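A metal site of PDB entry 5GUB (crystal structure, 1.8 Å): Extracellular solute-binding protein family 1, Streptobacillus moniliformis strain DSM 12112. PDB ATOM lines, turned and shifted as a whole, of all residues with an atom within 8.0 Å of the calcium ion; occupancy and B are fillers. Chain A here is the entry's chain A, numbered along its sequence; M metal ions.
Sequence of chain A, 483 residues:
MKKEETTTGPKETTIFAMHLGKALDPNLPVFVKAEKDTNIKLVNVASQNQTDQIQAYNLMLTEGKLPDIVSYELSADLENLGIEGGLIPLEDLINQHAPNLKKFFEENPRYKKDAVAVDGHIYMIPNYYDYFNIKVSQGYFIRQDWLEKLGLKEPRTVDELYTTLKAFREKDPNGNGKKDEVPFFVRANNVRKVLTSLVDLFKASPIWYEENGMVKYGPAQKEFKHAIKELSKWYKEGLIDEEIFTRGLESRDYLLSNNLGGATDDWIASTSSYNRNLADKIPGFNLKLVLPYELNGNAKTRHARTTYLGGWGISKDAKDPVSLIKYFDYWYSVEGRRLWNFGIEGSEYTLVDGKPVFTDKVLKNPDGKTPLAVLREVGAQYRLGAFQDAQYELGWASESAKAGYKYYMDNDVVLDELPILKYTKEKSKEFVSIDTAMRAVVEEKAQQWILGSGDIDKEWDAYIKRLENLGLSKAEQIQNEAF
OD2 of Asp 172 is in hydrogen-bond range of N of Gly 177 (2.8 Å).
The side-chain amide nitrogen (ND2) of Asn 174 sits at hydrogen-bond distance from the backbone carbonyl oxygen (O) of Asn 259, 2.9 Å away.
The backbone carbonyl oxygen of Glu 181 lies within hydrogen-bond range of the guanidinium group of Arg 169.
Six residues have an atom within 4 Å of the calcium ion: Asp 172, Asn 174, Asn 176, Lys 178, Asp 180 and Glu 181.
The nearest printed residue that does not touch the calcium ion is Lys 179 (4.6 Å).
The calcium ion is bound by the side-chain carboxylate (OD1) of Asp 172 (2.3 Å), the side-chain amide oxygen (OD1) of Asn 174 (2.3 Å), the backbone carbonyl oxygen (O) of Lys 178 (2.4 Å), the side-chain carboxylate (OD1) of Asp 180 (2.4 Å), the side-chain carboxylate (OE2) of Glu 181 (2.4 Å), the side-chain amide oxygen (OD1) of Asn 176 (2.5 Å) and the side-chain carboxylate (OE1) of Glu 181 (2.7 Å).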
ATOM      1  N   TRP A 146      32.383 -21.181  -7.154  1.00  0.00           N
ATOM      2  CA  TRP A 146      31.234 -22.012  -7.500  1.00  0.00           C
ATOM      3  C   TRP A 146      30.371 -21.332  -8.567  1.00  0.00           C
ATOM      4  O   TRP A 146      29.809 -22.006  -9.445  1.00  0.00           O
ATOM      5  CB  TRP A 146      30.407 -22.326  -6.254  1.00  0.00           C
ATOM      6  CG  TRP A 146      31.014 -23.390  -5.372  1.00  0.00           C
ATOM      7  CD1 TRP A 146      32.240 -23.976  -5.515  1.00  0.00           C
ATOM      8  CD2 TRP A 146      30.422 -23.969  -4.212  1.00  0.00           C
ATOM      9  NE1 TRP A 146      32.431 -24.904  -4.511  1.00  0.00           N
ATOM     10  CE2 TRP A 146      31.334 -24.916  -3.698  1.00  0.00           C
ATOM     11  CE3 TRP A 146      29.185 -23.795  -3.563  1.00  0.00           C
ATOM     12  CZ2 TRP A 146      31.061 -25.670  -2.565  1.00  0.00           C
ATOM     13  CZ3 TRP A 146      28.926 -24.554  -2.429  1.00  0.00           C
ATOM     14  CH2 TRP A 146      29.855 -25.479  -1.945  1.00  0.00           C
ATOM     15  N   PHE A 168      23.379 -24.227  -6.484  1.00  0.00           N
ATOM     16  CA  PHE A 168      24.400 -24.795  -5.595  1.00  0.00           C
ATOM     17  C   PHE A 168      23.978 -26.155  -5.037  1.00  0.00           C
ATOM     18  O   PHE A 168      24.777 -27.081  -4.914  1.00  0.00           O
ATOM     19  CB  PHE A 168      24.705 -23.837  -4.423  1.00  0.00           C
ATOM     20  CG  PHE A 168      25.524 -22.627  -4.796  1.00  0.00           C
ATOM     21  CD1 PHE A 168      25.999 -22.441  -6.077  1.00  0.00           C
ATOM     22  CD2 PHE A 168      25.837 -21.680  -3.823  1.00  0.00           C
ATOM     23  CE1 PHE A 168      26.768 -21.323  -6.401  1.00  0.00           C
ATOM     24  CE2 PHE A 168      26.602 -20.550  -4.141  1.00  0.00           C
ATOM     25  CZ  PHE A 168      27.072 -20.380  -5.427  1.00  0.00           C
ATOM     26  N   ARG A 169      22.693 -26.260  -4.685  1.00  0.00           N
ATOM     27  CA  ARG A 169      22.185 -27.470  -4.054  1.00  0.00           C
ATOM     28  C   ARG A 169      22.069 -28.603  -5.067  1.00  0.00           C
ATOM     29  O   ARG A 169      22.324 -29.766  -4.748  1.00  0.00           O
ATOM     30  CB  ARG A 169      20.828 -27.200  -3.396  1.00  0.00           C
ATOM     31  CG  ARG A 169      20.224 -28.415  -2.706  1.00  0.00           C
ATOM     32  CD  ARG A 169      21.156 -28.992  -1.618  1.00  0.00           C
ATOM     33  NE  ARG A 169      20.542 -30.163  -0.987  1.00  0.00           N
ATOM     34  CZ  ARG A 169      21.197 -31.054  -0.250  1.00  0.00           C
ATOM     35  NH1 ARG A 169      22.510 -30.933  -0.060  1.00  0.00           N
ATOM     36  NH2 ARG A 169      20.545 -32.097   0.267  1.00  0.00           N
ATOM     37  N   GLU A 170      21.693 -28.262  -6.296  1.00  0.00           N
ATOM     38  CA  GLU A 170      21.290 -29.295  -7.242  1.00  0.00           C
ATOM     39  C   GLU A 170      22.368 -29.675  -8.246  1.00  0.00           C
ATOM     40  O   GLU A 170      22.296 -30.751  -8.820  1.00  0.00           O
ATOM     41  CB  GLU A 170      20.033 -28.859  -7.996  1.00  0.00           C
ATOM     42  CG  GLU A 170      18.812 -28.635  -7.110  1.00  0.00           C
ATOM     43  CD  GLU A 170      18.370 -29.877  -6.339  1.00  0.00           C
ATOM     44  OE1 GLU A 170      18.654 -31.017  -6.793  1.00  0.00           O
ATOM     45  OE2 GLU A 170      17.747 -29.728  -5.260  1.00  0.00           O
ATOM     46  N   LYS A 171      23.346 -28.799  -8.460  1.00  0.00           N
ATOM     47  CA  LYS A 171      24.285 -28.996  -9.574  1.00  0.00           C
ATOM     48  C   LYS A 171      25.731 -29.282  -9.197  1.00  0.00           C
ATOM     49  O   LYS A 171      26.634 -29.109 -10.003  1.00  0.00           O
ATOM     50  CB  LYS A 171      24.203 -27.782 -10.510  1.00  0.00           C
ATOM     51  CG  LYS A 171      22.796 -27.587 -11.057  1.00  0.00           C
ATOM     52  CD  LYS A 171      22.654 -26.428 -12.024  1.00  0.00           C
ATOM     53  CE  LYS A 171      23.202 -26.799 -13.401  1.00  0.00           C
ATOM     54  NZ  LYS A 171      23.010 -25.712 -14.391  1.00  0.00           N
ATOM     55  N   ASP A 172      25.949 -29.736  -7.951  1.00  0.00           N
ATOM     56  CA  ASP A 172      27.250 -30.275  -7.534  1.00  0.00           C
ATOM     57  C   ASP A 172      28.451 -29.354  -7.816  1.00  0.00           C
ATOM     58  O   ASP A 172      29.411 -29.764  -8.481  1.00  0.00           O
ATOM     59  CB  ASP A 172      27.453 -31.654  -8.192  1.00  0.00           C
ATOM     60  CG  ASP A 172      28.659 -32.402  -7.658  1.00  0.00           C
ATOM     61  OD1 ASP A 172      28.947 -32.307  -6.447  1.00  0.00           O
ATOM     62  OD2 ASP A 172      29.339 -33.092  -8.451  1.00  0.00           O
ATOM     63  N   PRO A 173      28.412 -28.114  -7.313  1.00  0.00           N
ATOM     64  CA  PRO A 173      29.554 -27.237  -7.598  1.00  0.00           C
ATOM     65  C   PRO A 173      30.882 -27.707  -7.004  1.00  0.00           C
ATOM     66  O   PRO A 173      31.911 -27.351  -7.564  1.00  0.00           O
ATOM     67  CB  PRO A 173      29.121 -25.902  -6.958  1.00  0.00           C
ATOM     68  CG  PRO A 173      28.087 -26.276  -5.928  1.00  0.00           C
ATOM     69  CD  PRO A 173      27.355 -27.424  -6.561  1.00  0.00           C
ATOM     70  N   ASN A 174      30.907 -28.508  -5.938  1.00  0.00           N
ATOM     71  CA  ASN A 174      32.216 -28.929  -5.439  1.00  0.00           C
ATOM     72  C   ASN A 174      32.723 -30.162  -6.197  1.00  0.00           C
ATOM     73  O   ASN A 174      33.791 -30.695  -5.914  1.00  0.00           O
ATOM     74  CB  ASN A 174      32.212 -29.151  -3.901  1.00  0.00           C
ATOM     75  CG  ASN A 174      31.352 -30.320  -3.425  1.00  0.00           C
ATOM     76  OD1 ASN A 174      30.912 -31.185  -4.189  1.00  0.00           O
ATOM     77  ND2 ASN A 174      31.118 -30.356  -2.113  1.00  0.00           N
ATOM     78  N   GLY A 175      31.943 -30.598  -7.182  1.00  0.00           N
ATOM     79  CA  GLY A 175      32.399 -31.553  -8.176  1.00  0.00           C
ATOM     80  C   GLY A 175      32.630 -32.975  -7.722  1.00  0.00           C
ATOM     81  O   GLY A 175      33.294 -33.738  -8.433  1.00  0.00           O
ATOM     82  N   ASN A 176      32.077 -33.374  -6.580  1.00  0.00           N
ATOM     83  CA  ASN A 176      32.366 -34.719  -6.061  1.00  0.00           C
ATOM     84  C   ASN A 176      31.273 -35.743  -6.333  1.00  0.00           C
ATOM     85  O   ASN A 176      31.332 -36.879  -5.824  1.00  0.00           O
ATOM     86  CB  ASN A 176      32.670 -34.675  -4.562  1.00  0.00           C
ATOM     87  CG  ASN A 176      31.492 -34.167  -3.713  1.00  0.00           C
ATOM     88  OD1 ASN A 176      30.363 -34.016  -4.198  1.00  0.00           O
ATOM     89  ND2 ASN A 176      31.761 -33.952  -2.441  1.00  0.00           N
ATOM     90  N   GLY A 177      30.278 -35.363  -7.127  1.00  0.00           N
ATOM     91  CA  GLY A 177      29.190 -36.264  -7.491  1.00  0.00           C
ATOM     92  C   GLY A 177      28.204 -36.557  -6.377  1.00  0.00           C
ATOM     93  O   GLY A 177      27.342 -37.407  -6.509  1.00  0.00           O
ATOM     94  N   LYS A 178      28.325 -35.834  -5.256  1.00  0.00           N
ATOM     95  CA  LYS A 178      27.430 -36.002  -4.130  1.00  0.00           C
ATOM     96  C   LYS A 178      26.578 -34.755  -3.926  1.00  0.00           C
ATOM     97  O   LYS A 178      27.069 -33.639  -4.089  1.00  0.00           O
ATOM     98  CB  LYS A 178      28.203 -36.275  -2.833  1.00  0.00           C
ATOM     99  CG  LYS A 178      29.105 -37.506  -2.873  1.00  0.00           C
ATOM    100  CD  LYS A 178      29.674 -37.783  -1.493  1.00  0.00           C
ATOM    101  CE  LYS A 178      30.486 -39.068  -1.487  1.00  0.00           C
ATOM    102  NZ  LYS A 178      31.796 -38.891  -2.158  1.00  0.00           N
ATOM    103  N   LYS A 179      25.332 -34.956  -3.537  1.00  0.00           N
ATOM    104  CA  LYS A 179      24.459 -33.846  -3.193  1.00  0.00           C
ATOM    105  C   LYS A 179      24.727 -33.468  -1.738  1.00  0.00           C
ATOM    106  O   LYS A 179      23.909 -33.741  -0.841  1.00  0.00           O
ATOM    107  CB  LYS A 179      22.994 -34.226  -3.383  1.00  0.00           C
ATOM    108  CG  LYS A 179      22.017 -33.063  -3.421  1.00  0.00           C
ATOM    109  CD  LYS A 179      20.630 -33.606  -3.647  1.00  0.00           C
ATOM    110  CE  LYS A 179      19.578 -32.533  -3.594  1.00  0.00           C
ATOM    111  NZ  LYS A 179      18.216 -33.151  -3.802  1.00  0.00           N
ATOM    112  N   ASP A 180      25.887 -32.864  -1.507  1.00  0.00           N
ATOM    113  CA  ASP A 180      26.312 -32.599  -0.131  1.00  0.00           C
ATOM    114  C   ASP A 180      26.392 -31.105   0.150  1.00  0.00           C
ATOM    115  O   ASP A 180      26.674 -30.712   1.277  1.00  0.00           O
ATOM    116  CB  ASP A 180      27.664 -33.279   0.125  1.00  0.00           C
ATOM    117  CG  ASP A 180      28.771 -32.793  -0.801  1.00  0.00           C
ATOM    118  OD1 ASP A 180      28.493 -32.168  -1.854  1.00  0.00           O
ATOM    119  OD2 ASP A 180      29.951 -33.064  -0.485  1.00  0.00           O
ATOM    120  N   GLU A 181      26.118 -30.298  -0.867  1.00  0.00           N
ATOM    121  CA  GLU A 181      26.246 -28.842  -0.755  1.00  0.00           C
ATOM    122  C   GLU A 181      25.271 -28.260   0.262  1.00  0.00           C
ATOM    123  O   GLU A 181      24.112 -28.670   0.353  1.00  0.00           O
ATOM    124  CB  GLU A 181      26.059 -28.195  -2.132  1.00  0.00           C
ATOM    125  CG  GLU A 181      27.329 -28.238  -2.984  1.00  0.00           C
ATOM    126  CD  GLU A 181      27.581 -29.571  -3.683  1.00  0.00           C
ATOM    127  OE1 GLU A 181      26.746 -30.494  -3.573  1.00  0.00           O
ATOM    128  OE2 GLU A 181      28.636 -29.686  -4.328  1.00  0.00           O
ATOM    129  N   VAL A 182      25.780 -27.315   1.046  1.00  0.00           N
ATOM    130  CA  VAL A 182      24.993 -26.540   1.993  1.00  0.00           C
ATOM    131  C   VAL A 182      25.024 -25.107   1.483  1.00  0.00           C
ATOM    132  O   VAL A 182      25.974 -24.380   1.768  1.00  0.00           O
ATOM    133  CB  VAL A 182      25.557 -26.636   3.420  1.00  0.00           C
ATOM    134  CG1 VAL A 182      24.760 -25.755   4.379  1.00  0.00           C
ATOM    135  CG2 VAL A 182      25.552 -28.096   3.886  1.00  0.00           C
ATOM    136  N   ASN A 259      34.468 -27.863   2.195  1.00  0.00           N
ATOM    137  CA  ASN A 259      33.983 -27.450   0.867  1.00  0.00           C
ATOM    138  C   ASN A 259      32.518 -27.772   0.642  1.00  0.00           C
ATOM    139  O   ASN A 259      32.129 -28.230  -0.444  1.00  0.00           O
ATOM    140  CB  ASN A 259      34.821 -28.116  -0.242  1.00  0.00           C
ATOM    141  CG  ASN A 259      34.808 -27.317  -1.523  1.00  0.00           C
ATOM    142  OD1 ASN A 259      34.442 -26.133  -1.535  1.00  0.00           O
ATOM    143  ND2 ASN A 259      35.195 -27.968  -2.624  1.00  0.00           N
ATOM    144  N   LEU A 260      31.704 -27.519   1.666  1.00  0.00           N
ATOM    145  CA  LEU A 260      30.263 -27.738   1.616  1.00  0.00           C
ATOM    146  C   LEU A 260      29.456 -26.444   1.499  1.00  0.00           C
ATOM    147  O   LEU A 260      28.384 -26.431   0.884  1.00  0.00           O
ATOM    148  CB  LEU A 260      29.783 -28.475   2.866  1.00  0.00           C
ATOM    149  CG  LEU A 260      30.469 -29.804   3.184  1.00  0.00           C
ATOM    150  CD1 LEU A 260      29.914 -30.342   4.498  1.00  0.00           C
ATOM    151  CD2 LEU A 260      30.285 -30.795   2.042  1.00  0.00           C
HETATM  152 CA    CA M   1      28.805 -32.057  -4.186  1.00  0.00          CA
